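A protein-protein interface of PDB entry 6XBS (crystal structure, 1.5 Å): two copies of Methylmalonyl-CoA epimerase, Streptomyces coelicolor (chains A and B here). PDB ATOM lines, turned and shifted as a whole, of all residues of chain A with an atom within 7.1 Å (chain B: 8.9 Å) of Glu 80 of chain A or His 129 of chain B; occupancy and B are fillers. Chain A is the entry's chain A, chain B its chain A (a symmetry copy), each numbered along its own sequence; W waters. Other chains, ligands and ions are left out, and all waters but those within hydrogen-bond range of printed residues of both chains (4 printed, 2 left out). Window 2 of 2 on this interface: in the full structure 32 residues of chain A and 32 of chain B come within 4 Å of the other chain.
Thr 18 of chain A touches His 129 of chain B.
Phe 21 of chain A touches Asp 127 of chain B.
CZ of Phe 21 of chain A touches CA of Cys 128 of chain B (3.6 Å).
Phe 21 of chain A touches His 129 of chain B.
Glu 80 of chain A touches Gly 130 of chain B (O to CA, 3.4 Å).
His 129 of chain B touches Gly 81 of chain A (O to N, 3.7 Å).
Gly 81 of chain A touches Gly 130 of chain B (CA to O, 3.7 Å).
Val 131 of chain B touches Gly 81 of chain A (CG2 to CA, 3.95 Å).
Printed residues of chain A that touch a printed residue of chain B: Thr 18, Phe 21, Glu 80 and Gly 81.
Hydrophobic or aromatic side chains of chain A within 4 Å of the printed part of chain B: Phe 21.
Printed residues of chain B that touch a printed residue of chain A: Asp 127, Cys 128, His 129, Gly 130 and Val 131.
No position is printed for both chains.
Glu 80 of chain A touches two residues of chain B.
Of chain A, only Thr 18 (3.8 Å), Phe 21 (3.8 Å), Glu 80 (2.8 Å) and Gly 81 (3.7 Å) come within 4 Å of His 129 of chain B.
No residue of chain B comes within 4 Å of Gly 79 of chain A.
Gly 81 of chain A touches just these residues of chain B: His 129, Gly 130 and Val 131.
Printed residues of chain A within 4 Å of Asp 127 of chain B: Phe 21.
Of the printed residues of chain B, Thr 18 of chain A touches His 129.
Printed residues of chain A within 4 Å of Val 131 of chain B: Gly 81 (3.95 Å).
Of the printed residues of chain A, Cys 128 of chain B touches Phe 21 (3.6 Å).
Printed residues of chain B within 4 Å of Phe 21 of chain A: Asp 127 (3.2 Å), Cys 128 (3.6 Å) and His 129 (3.8 Å).
The nearest residue of chain B that does not touch Glu 80 of chain A is Val 131 of chain B (5.1 Å).
The nearest residue of chain A that does not touch His 129 of chain B is Ala 17 of chain A (4.4 Å).
The nearest printed residue of chain A that does not touch Asp 127 of chain B is Tyr 22 of chain A (8.0 Å).
The backbone carbonyl oxygen (O) of Val 131 of chain B lies within hydrogen-bond range of the side-chain hydroxyl (OG1) of Thr 133 of chain B, at 2.9 Å.
The backbone carbonyl oxygen (O) of His 124 of chain B lies within hydrogen-bond range of the side-chain sulfur (SG) of Cys 128 of chain B (3.5 Å).
O of Pro 125 of chain B lies within hydrogen-bond range of N of Gly 130 of chain B (2.8 Å).
The backbone NH of Ala 11 of chain A is in hydrogen-bond range of the backbone carbonyl oxygen of Gly 81 of chain A (2.9 Å).
O of Asp 14 of chain A is in hydrogen-bond range of OG1 of Thr 18 of chain A (3.1 Å).
SG of Cys 12 of chain A sits close to OG1 of Thr 18 of chain A (3.6 Å).
The side-chain carboxylate of Glu 80 of chain A is in hydrogen-bond range of a ring nitrogen (ND1) of His 129 of chain B.
Water W1 bridges the side-chain hydroxyl (OH) of Tyr 22 of chain A (2.6 Å) and the backbone carbonyl oxygen (O) of Cys 128 of chain B (2.8 Å).
Water W3 bridges the backbone carbonyl oxygen (O) of Gly 130 of chain B and the backbone carbonyl oxygen (O) of Glu 80 of chain A.
Water W2 lies within hydrogen-bond range of O of His 129 of chain B (2.7 Å) and O of Ala 11 of chain A (3.0 Å).
Water W4 lies within hydrogen-bond range of OG1 of Thr 133 of chain B (2.8 Å) and OH of Tyr 22 of chain A (3.0 Å).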
ATOM      1  N   ILE A  10       5.474 -31.019  21.467  1.00  0.00           N
ATOM      2  CA  ILE A  10       4.238 -30.396  20.947  1.00  0.00           C
ATOM      3  C   ILE A  10       3.127 -31.416  20.969  1.00  0.00           C
ATOM      4  O   ILE A  10       3.285 -32.470  20.315  1.00  0.00           O
ATOM      5  CB  ILE A  10       4.503 -29.878  19.533  1.00  0.00           C
ATOM      6  CG1 ILE A  10       5.569 -28.770  19.571  1.00  0.00           C
ATOM      7  CG2 ILE A  10       3.222 -29.423  18.875  1.00  0.00           C
ATOM      8  CD1 ILE A  10       6.057 -28.337  18.231  1.00  0.00           C
ATOM      9  N   ALA A  11       2.069 -31.154  21.728  1.00  0.00           N
ATOM     10  CA  ALA A  11       0.901 -32.058  21.837  1.00  0.00           C
ATOM     11  C   ALA A  11      -0.064 -31.796  20.686  1.00  0.00           C
ATOM     12  O   ALA A  11      -0.348 -30.639  20.328  1.00  0.00           O
ATOM     13  CB  ALA A  11       0.225 -31.853  23.188  1.00  0.00           C
ATOM     14  N   CYS A  12      -0.608 -32.892  20.173  1.00  0.00           N
ATOM     15  CA  CYS A  12      -1.580 -32.834  19.082  1.00  0.00           C
ATOM     16  C   CYS A  12      -2.602 -33.954  19.230  1.00  0.00           C
ATOM     17  O   CYS A  12      -2.343 -34.976  19.791  1.00  0.00           O
ATOM     18  CB  CYS A  12      -0.901 -32.812  17.722  1.00  0.00           C
ATOM     19  SG  CYS A  12       0.057 -34.311  17.370  1.00  0.00           S
ATOM     20  N   HIS A  13      -3.730 -33.699  18.607  1.00  0.00           N
ATOM     21  CA  HIS A  13      -4.824 -34.699  18.656  1.00  0.00           C
ATOM     22  C   HIS A  13      -4.587 -35.836  17.666  1.00  0.00           C
ATOM     23  O   HIS A  13      -4.929 -37.011  17.985  1.00  0.00           O
ATOM     24  CB  HIS A  13      -6.130 -33.992  18.274  1.00  0.00           C
ATOM     25  CG  HIS A  13      -6.657 -33.065  19.311  1.00  0.00           C
ATOM     26  ND1 HIS A  13      -6.907 -33.481  20.586  1.00  0.00           N
ATOM     27  CD2 HIS A  13      -7.003 -31.787  19.240  1.00  0.00           C
ATOM     28  CE1 HIS A  13      -7.368 -32.465  21.272  1.00  0.00           C
ATOM     29  NE2 HIS A  13      -7.423 -31.429  20.477  1.00  0.00           N
ATOM     30  N   ASP A  14      -3.980 -35.534  16.518  1.00  0.00           N
ATOM     31  CA  ASP A  14      -3.763 -36.505  15.430  1.00  0.00           C
ATOM     32  C   ASP A  14      -2.311 -36.389  14.947  1.00  0.00           C
ATOM     33  O   ASP A  14      -1.987 -35.476  14.175  1.00  0.00           O
ATOM     34  CB  ASP A  14      -4.802 -36.263  14.343  1.00  0.00           C
ATOM     35  CG  ASP A  14      -4.774 -37.152  13.124  1.00  0.00           C
ATOM     36  OD1 ASP A  14      -3.786 -37.805  12.833  1.00  0.00           O
ATOM     37  OD2 ASP A  14      -5.825 -37.067  12.370  1.00  0.00           O
ATOM     38  N   LEU A  15      -1.521 -37.352  15.355  1.00  0.00           N
ATOM     39  CA  LEU A  15      -0.091 -37.327  15.022  1.00  0.00           C
ATOM     40  C   LEU A  15       0.090 -37.316  13.501  1.00  0.00           C
ATOM     41  O   LEU A  15       0.900 -36.544  12.972  1.00  0.00           O
ATOM     42  CB  LEU A  15       0.619 -38.505  15.642  1.00  0.00           C
ATOM     43  CG  LEU A  15       2.126 -38.519  15.431  1.00  0.00           C
ATOM     44  CD1 LEU A  15       2.775 -37.322  16.109  1.00  0.00           C
ATOM     45  CD2 LEU A  15       2.743 -39.772  15.960  1.00  0.00           C
ATOM     46  N   ALA A  17      -1.785 -36.282  11.024  1.00  0.00           N
ATOM     47  CA  ALA A  17      -2.197 -35.013  10.417  1.00  0.00           C
ATOM     48  C   ALA A  17      -1.177 -33.897  10.742  1.00  0.00           C
ATOM     49  O   ALA A  17      -0.846 -33.066   9.891  1.00  0.00           O
ATOM     50  CB  ALA A  17      -3.565 -34.594  10.882  1.00  0.00           C
ATOM     51  N   THR A  18      -0.697 -33.924  11.982  1.00  0.00           N
ATOM     52  CA  THR A  18       0.224 -32.834  12.393  1.00  0.00           C
ATOM     53  C   THR A  18       1.605 -33.077  11.775  1.00  0.00           C
ATOM     54  O   THR A  18       2.243 -32.091  11.305  1.00  0.00           O
ATOM     55  CB  THR A  18       0.252 -32.762  13.908  1.00  0.00           C
ATOM     56  OG1 THR A  18      -1.061 -32.565  14.457  1.00  0.00           O
ATOM     57  CG2 THR A  18       1.093 -31.591  14.378  1.00  0.00           C
ATOM     58  N   VAL A  19       2.096 -34.306  11.712  1.00  0.00           N
ATOM     59  CA  VAL A  19       3.294 -34.652  10.929  1.00  0.00           C
ATOM     60  C   VAL A  19       3.180 -34.119   9.499  1.00  0.00           C
ATOM     61  O   VAL A  19       4.121 -33.484   9.002  1.00  0.00           O
ATOM     62  CB  VAL A  19       3.580 -36.161  11.015  1.00  0.00           C
ATOM     63  CG1 VAL A  19       4.517 -36.627   9.939  1.00  0.00           C
ATOM     64  CG2 VAL A  19       4.103 -36.593  12.370  1.00  0.00           C
ATOM     65  N   GLU A  20       2.047 -34.383   8.846  1.00  0.00           N
ATOM     66  CA  GLU A  20       1.848 -33.931   7.466  1.00  0.00           C
ATOM     67  C   GLU A  20       1.894 -32.409   7.370  1.00  0.00           C
ATOM     68  O   GLU A  20       2.485 -31.885   6.437  1.00  0.00           O
ATOM     69  CB  GLU A  20       0.553 -34.520   6.934  1.00  0.00           C
ATOM     70  CG  GLU A  20       0.284 -34.051   5.511  1.00  0.00           C
ATOM     71  CD  GLU A  20       1.322 -34.313   4.432  1.00  0.00           C
ATOM     72  OE1 GLU A  20       2.250 -35.168   4.597  1.00  0.00           O
ATOM     73  OE2 GLU A  20       1.260 -33.596   3.426  1.00  0.00           O
ATOM     74  N   PHE A  21       1.306 -31.718   8.335  1.00  0.00           N
ATOM     75  CA  PHE A  21       1.373 -30.259   8.401  1.00  0.00           C
ATOM     76  C   PHE A  21       2.824 -29.748   8.403  1.00  0.00           C
ATOM     77  O   PHE A  21       3.223 -28.870   7.667  1.00  0.00           O
ATOM     78  CB  PHE A  21       0.578 -29.686   9.583  1.00  0.00           C
ATOM     79  CG  PHE A  21       0.868 -28.247   9.834  1.00  0.00           C
ATOM     80  CD1 PHE A  21       0.322 -27.284   9.014  1.00  0.00           C
ATOM     81  CD2 PHE A  21       1.758 -27.833  10.813  1.00  0.00           C
ATOM     82  CE1 PHE A  21       0.620 -25.946   9.209  1.00  0.00           C
ATOM     83  CE2 PHE A  21       2.081 -26.491  10.936  1.00  0.00           C
ATOM     84  CZ  PHE A  21       1.530 -25.580  10.127  1.00  0.00           C
ATOM     85  N   TYR A  22       3.653 -30.358   9.254  1.00  0.00           N
ATOM     86  CA  TYR A  22       5.064 -29.888   9.368  1.00  0.00           C
ATOM     87  C   TYR A  22       5.838 -30.235   8.096  1.00  0.00           C
ATOM     88  O   TYR A  22       6.681 -29.451   7.665  1.00  0.00           O
ATOM     89  CB  TYR A  22       5.725 -30.446  10.659  1.00  0.00           C
ATOM     90  CG  TYR A  22       5.406 -29.632  11.894  1.00  0.00           C
ATOM     91  CD1 TYR A  22       4.285 -29.861  12.652  1.00  0.00           C
ATOM     92  CD2 TYR A  22       6.180 -28.543  12.243  1.00  0.00           C
ATOM     93  CE1 TYR A  22       3.904 -29.082  13.724  1.00  0.00           C
ATOM     94  CE2 TYR A  22       5.801 -27.695  13.253  1.00  0.00           C
ATOM     95  CZ  TYR A  22       4.689 -27.966  14.012  1.00  0.00           C
ATOM     96  OH  TYR A  22       4.315 -27.123  15.015  1.00  0.00           O
ATOM     97  N   TRP A  74      -3.622 -32.942  29.512  1.00  0.00           N
ATOM     98  CA  TRP A  74      -3.239 -31.587  29.124  1.00  0.00           C
ATOM     99  C   TRP A  74      -3.975 -31.127  27.868  1.00  0.00           C
ATOM    100  O   TRP A  74      -4.410 -29.972  27.795  1.00  0.00           O
ATOM    101  CB  TRP A  74      -1.705 -31.574  28.958  1.00  0.00           C
ATOM    102  CG  TRP A  74      -1.174 -30.208  28.747  1.00  0.00           C
ATOM    103  CD1 TRP A  74      -0.714 -29.359  29.697  1.00  0.00           C
ATOM    104  CD2 TRP A  74      -1.000 -29.551  27.507  1.00  0.00           C
ATOM    105  NE1 TRP A  74      -0.346 -28.186  29.142  1.00  0.00           N
ATOM    106  CE2 TRP A  74      -0.480 -28.282  27.785  1.00  0.00           C
ATOM    107  CE3 TRP A  74      -1.249 -29.894  26.181  1.00  0.00           C
ATOM    108  CZ2 TRP A  74      -0.188 -27.372  26.802  1.00  0.00           C
ATOM    109  CZ3 TRP A  74      -0.971 -28.985  25.197  1.00  0.00           C
ATOM    110  CH2 TRP A  74      -0.432 -27.757  25.502  1.00  0.00           C
ATOM    111  N   LEU A  75      -4.113 -31.988  26.871  1.00  0.00           N
ATOM    112  CA  LEU A  75      -4.809 -31.621  25.624  1.00  0.00           C
ATOM    113  C   LEU A  75      -6.283 -31.320  25.926  1.00  0.00           C
ATOM    114  O   LEU A  75      -6.832 -30.408  25.313  1.00  0.00           O
ATOM    115  CB  LEU A  75      -4.759 -32.751  24.592  1.00  0.00           C
ATOM    116  CG  LEU A  75      -3.536 -32.778  23.714  1.00  0.00           C
ATOM    117  CD1 LEU A  75      -3.506 -34.075  22.917  1.00  0.00           C
ATOM    118  CD2 LEU A  75      -3.591 -31.593  22.770  1.00  0.00           C
ATOM    119  N   ALA A  76      -6.876 -32.112  26.823  1.00  0.00           N
ATOM    120  CA  ALA A  76      -8.316 -31.923  27.128  1.00  0.00           C
ATOM    121  C   ALA A  76      -8.521 -30.536  27.735  1.00  0.00           C
ATOM    122  O   ALA A  76      -9.509 -29.845  27.403  1.00  0.00           O
ATOM    123  CB  ALA A  76      -8.784 -33.040  28.036  1.00  0.00           C
ATOM    124  N   ASN A  78      -6.247 -27.835  27.509  1.00  0.00           N
ATOM    125  CA  ASN A  78      -5.594 -26.655  26.901  1.00  0.00           C
ATOM    126  C   ASN A  78      -5.696 -26.609  25.363  1.00  0.00           C
ATOM    127  O   ASN A  78      -5.367 -25.547  24.801  1.00  0.00           O
ATOM    128  CB  ASN A  78      -4.101 -26.706  27.249  1.00  0.00           C
ATOM    129  CG  ASN A  78      -3.861 -26.542  28.732  1.00  0.00           C
ATOM    130  OD1 ASN A  78      -4.043 -25.441  29.265  1.00  0.00           O
ATOM    131  ND2 ASN A  78      -3.528 -27.630  29.386  1.00  0.00           N
ATOM    132  N   GLY A  79      -6.039 -27.706  24.712  1.00  0.00           N
ATOM    133  CA  GLY A  79      -5.963 -27.839  23.260  1.00  0.00           C
ATOM    134  C   GLY A  79      -4.517 -28.010  22.785  1.00  0.00           C
ATOM    135  O   GLY A  79      -3.623 -28.036  23.618  1.00  0.00           O
ATOM    136  N   GLU A  80      -4.374 -28.193  21.500  1.00  0.00           N
ATOM    137  CA  GLU A  80      -3.066 -28.491  20.890  1.00  0.00           C
ATOM    138  C   GLU A  80      -2.130 -27.297  21.105  1.00  0.00           C
ATOM    139  O   GLU A  80      -2.496 -26.143  21.090  1.00  0.00           O
ATOM    140  CB  GLU A  80      -3.237 -28.644  19.381  1.00  0.00           C
ATOM    141  CG  GLU A  80      -4.163 -29.758  18.947  1.00  0.00           C
ATOM    142  CD  GLU A  80      -4.069 -30.095  17.476  1.00  0.00           C
ATOM    143  OE1 GLU A  80      -4.252 -29.172  16.648  1.00  0.00           O
ATOM    144  OE2 GLU A  80      -3.895 -31.287  17.215  1.00  0.00           O
ATOM    145  N   GLY A  81      -0.832 -27.646  21.236  1.00  0.00           N
ATOM    146  CA  GLY A  81       0.232 -26.626  21.365  1.00  0.00           C
ATOM    147  C   GLY A  81       1.448 -27.177  22.079  1.00  0.00           C
ATOM    148  O   GLY A  81       1.626 -28.380  22.267  1.00  0.00           O
ATOM    149  N   VAL A  82       2.332 -26.264  22.442  1.00  0.00           N
ATOM    150  CA  VAL A  82       3.583 -26.663  23.126  1.00  0.00           C
ATOM    151  C   VAL A  82       3.311 -27.209  24.509  1.00  0.00           C
ATOM    152  O   VAL A  82       2.656 -26.467  25.322  1.00  0.00           O
ATOM    153  CB  VAL A  82       4.579 -25.503  23.170  1.00  0.00           C
ATOM    154  CG1 VAL A  82       5.832 -25.889  23.936  1.00  0.00           C
ATOM    155  CG2 VAL A  82       4.974 -24.978  21.798  1.00  0.00           C
ATOM    156  N   HIS A  83       3.786 -28.386  24.774  1.00  0.00           N
ATOM    157  CA  HIS A  83       3.591 -29.059  26.063  1.00  0.00           C
ATOM    158  C   HIS A  83       4.831 -28.974  26.937  1.00  0.00           C
ATOM    159  O   HIS A  83       4.689 -28.860  28.152  1.00  0.00           O
ATOM    160  CB  HIS A  83       3.163 -30.491  25.804  1.00  0.00           C
ATOM    161  CG  HIS A  83       3.022 -31.294  27.053  1.00  0.00           C
ATOM    162  ND1 HIS A  83       3.965 -32.217  27.433  1.00  0.00           N
ATOM    163  CD2 HIS A  83       2.067 -31.282  28.029  1.00  0.00           C
ATOM    164  CE1 HIS A  83       3.587 -32.761  28.587  1.00  0.00           C
ATOM    165  NE2 HIS A  83       2.418 -32.228  28.974  1.00  0.00           N
ATOM    166  N   VAL B 104      -1.434 -20.723   4.996  1.00  0.00           N
ATOM    167  CA  VAL B 104      -1.130 -20.402   6.411  1.00  0.00           C
ATOM    168  C   VAL B 104      -1.025 -18.904   6.571  1.00  0.00           C
ATOM    169  O   VAL B 104      -0.337 -18.243   5.777  1.00  0.00           O
ATOM    170  CB  VAL B 104       0.198 -21.069   6.839  1.00  0.00           C
ATOM    171  CG1 VAL B 104       0.635 -20.604   8.234  1.00  0.00           C
ATOM    172  CG2 VAL B 104       0.050 -22.578   6.802  1.00  0.00           C
ATOM    173  N   LEU B 123       3.442 -16.761  12.048  1.00  0.00           N
ATOM    174  CA  LEU B 123       2.355 -17.570  11.494  1.00  0.00           C
ATOM    175  C   LEU B 123       1.286 -17.716  12.529  1.00  0.00           C
ATOM    176  O   LEU B 123       1.522 -18.012  13.694  1.00  0.00           O
ATOM    177  CB  LEU B 123       2.856 -18.921  11.030  1.00  0.00           C
ATOM    178  CG  LEU B 123       4.129 -18.901  10.184  1.00  0.00           C
ATOM    179  CD1 LEU B 123       4.601 -20.264   9.791  1.00  0.00           C
ATOM    180  CD2 LEU B 123       3.935 -18.055   8.931  1.00  0.00           C
ATOM    181  N   HIS B 124       0.007 -17.636  12.118  1.00  0.00           N
ATOM    182  CA  HIS B 124      -1.107 -17.687  13.070  1.00  0.00           C
ATOM    183  C   HIS B 124      -1.194 -19.044  13.754  1.00  0.00           C
ATOM    184  O   HIS B 124      -1.188 -20.072  13.079  1.00  0.00           O
ATOM    185  CB  HIS B 124      -2.435 -17.379  12.318  1.00  0.00           C
ATOM    186  CG  HIS B 124      -3.501 -16.957  13.260  1.00  0.00           C
ATOM    187  ND1 HIS B 124      -4.055 -17.802  14.206  1.00  0.00           N
ATOM    188  CD2 HIS B 124      -4.087 -15.743  13.431  1.00  0.00           C
ATOM    189  CE1 HIS B 124      -4.988 -17.112  14.896  1.00  0.00           C
ATOM    190  NE2 HIS B 124      -5.001 -15.868  14.444  1.00  0.00           N
ATOM    191  N   PRO B 125      -1.281 -19.101  15.114  1.00  0.00           N
ATOM    192  CA  PRO B 125      -1.314 -20.374  15.800  1.00  0.00           C
ATOM    193  C   PRO B 125      -2.465 -21.266  15.400  1.00  0.00           C
ATOM    194  O   PRO B 125      -2.350 -22.498  15.437  1.00  0.00           O
ATOM    195  CB  PRO B 125      -1.381 -19.969  17.276  1.00  0.00           C
ATOM    196  CG  PRO B 125      -1.893 -18.561  17.272  1.00  0.00           C
ATOM    197  CD  PRO B 125      -1.331 -17.953  16.011  1.00  0.00           C
ATOM    198  N   LYS B 126      -3.593 -20.630  15.006  1.00  0.00           N
ATOM    199  CA  LYS B 126      -4.728 -21.474  14.649  1.00  0.00           C
ATOM    200  C   LYS B 126      -4.526 -22.157  13.315  1.00  0.00           C
ATOM    201  O   LYS B 126      -5.269 -23.135  13.011  1.00  0.00           O
ATOM    202  CB  LYS B 126      -6.003 -20.628  14.609  1.00  0.00           C
ATOM    203  CG  LYS B 126      -6.419 -20.082  15.946  1.00  0.00           C
ATOM    204  CD  LYS B 126      -6.809 -21.121  16.960  1.00  0.00           C
ATOM    205  CE  LYS B 126      -8.136 -21.771  16.646  1.00  0.00           C
ATOM    206  NZ  LYS B 126      -9.220 -20.768  16.480  1.00  0.00           N
ATOM    207  N   ASP B 127      -3.540 -21.786  12.540  1.00  0.00           N
ATOM    208  CA  ASP B 127      -3.143 -22.474  11.302  1.00  0.00           C
ATOM    209  C   ASP B 127      -1.960 -23.408  11.509  1.00  0.00           C
ATOM    210  O   ASP B 127      -1.569 -24.105  10.565  1.00  0.00           O
ATOM    211  CB  ASP B 127      -2.807 -21.481  10.215  1.00  0.00           C
ATOM    212  CG  ASP B 127      -3.964 -20.588   9.781  1.00  0.00           C
ATOM    213  OD1 ASP B 127      -5.142 -20.963  10.105  1.00  0.00           O
ATOM    214  OD2 ASP B 127      -3.727 -19.591   9.114  1.00  0.00           O
ATOM    215  N   CYS B 128      -1.406 -23.435  12.729  1.00  0.00           N
ATOM    216  CA  CYS B 128      -0.171 -24.218  13.024  1.00  0.00           C
ATOM    217  C   CYS B 128      -0.451 -25.195  14.170  1.00  0.00           C
ATOM    218  O   CYS B 128       0.426 -25.426  15.034  1.00  0.00           O
ATOM    219  CB  CYS B 128       0.993 -23.310  13.376  1.00  0.00           C
ATOM    220  SG  CYS B 128       1.452 -22.169  12.059  1.00  0.00           S
ATOM    221  N   HIS B 129      -1.676 -25.729  14.290  1.00  0.00           N
ATOM    222  CA  HIS B 129      -2.006 -26.709  15.345  1.00  0.00           C
ATOM    223  C   HIS B 129      -1.663 -26.112  16.704  1.00  0.00           C
ATOM    224  O   HIS B 129      -1.174 -26.838  17.597  1.00  0.00           O
ATOM    225  CB  HIS B 129      -1.357 -28.060  15.017  1.00  0.00           C
ATOM    226  CG  HIS B 129      -1.970 -28.770  13.852  1.00  0.00           C
ATOM    227  ND1 HIS B 129      -3.165 -29.452  14.082  1.00  0.00           N
ATOM    228  CD2 HIS B 129      -1.697 -28.811  12.557  1.00  0.00           C
ATOM    229  CE1 HIS B 129      -3.544 -29.934  12.894  1.00  0.00           C
ATOM    230  NE2 HIS B 129      -2.665 -29.599  11.943  1.00  0.00           N
ATOM    231  N   GLY B 130      -1.972 -24.851  16.966  1.00  0.00           N
ATOM    232  CA  GLY B 130      -1.936 -24.245  18.293  1.00  0.00           C
ATOM    233  C   GLY B 130      -0.596 -23.647  18.674  1.00  0.00           C
ATOM    234  O   GLY B 130      -0.461 -23.290  19.835  1.00  0.00           O
ATOM    235  N   VAL B 131       0.369 -23.610  17.743  1.00  0.00           N
ATOM    236  CA  VAL B 131       1.719 -23.106  18.082  1.00  0.00           C
ATOM    237  C   VAL B 131       1.963 -21.795  17.343  1.00  0.00           C
ATOM    238  O   VAL B 131       1.943 -21.771  16.082  1.00  0.00           O
ATOM    239  CB  VAL B 131       2.791 -24.146  17.692  1.00  0.00           C
ATOM    240  CG1 VAL B 131       4.192 -23.569  17.979  1.00  0.00           C
ATOM    241  CG2 VAL B 131       2.571 -25.458  18.398  1.00  0.00           C
ATOM    242  N   LEU B 132       2.089 -20.701  18.079  1.00  0.00           N
ATOM    243  CA  LEU B 132       2.498 -19.437  17.461  1.00  0.00           C
ATOM    244  C   LEU B 132       3.934 -19.627  16.961  1.00  0.00           C
ATOM    245  O   LEU B 132       4.808 -19.949  17.779  1.00  0.00           O
ATOM    246  CB  LEU B 132       2.387 -18.284  18.443  1.00  0.00           C
ATOM    247  CG  LEU B 132       2.891 -16.942  17.975  1.00  0.00           C
ATOM    248  CD1 LEU B 132       2.201 -16.369  16.726  1.00  0.00           C
ATOM    249  CD2 LEU B 132       2.782 -15.926  19.105  1.00  0.00           C
ATOM    250  N   THR B 133       4.155 -19.426  15.689  1.00  0.00           N
ATOM    251  CA  THR B 133       5.413 -19.832  15.036  1.00  0.00           C
ATOM    252  C   THR B 133       6.053 -18.619  14.421  1.00  0.00           C
ATOM    253  O   THR B 133       5.467 -17.948  13.553  1.00  0.00           O
ATOM    254  CB  THR B 133       5.165 -20.936  14.027  1.00  0.00           C
ATOM    255  OG1 THR B 133       4.527 -22.040  14.695  1.00  0.00           O
ATOM    256  CG2 THR B 133       6.438 -21.381  13.350  1.00  0.00           C
HETATM  257  O   HOH W   1       1.921 -27.627  15.993  1.00  0.00           O
HETATM  258  O   HOH W   2       0.264 -29.168  17.835  1.00  0.00           O
HETATM  259  O   HOH W   3      -1.842 -23.339  22.202  1.00  0.00           O
HETATM  260  O   HOH W   4       4.365 -24.536  13.480  1.00  0.00           O
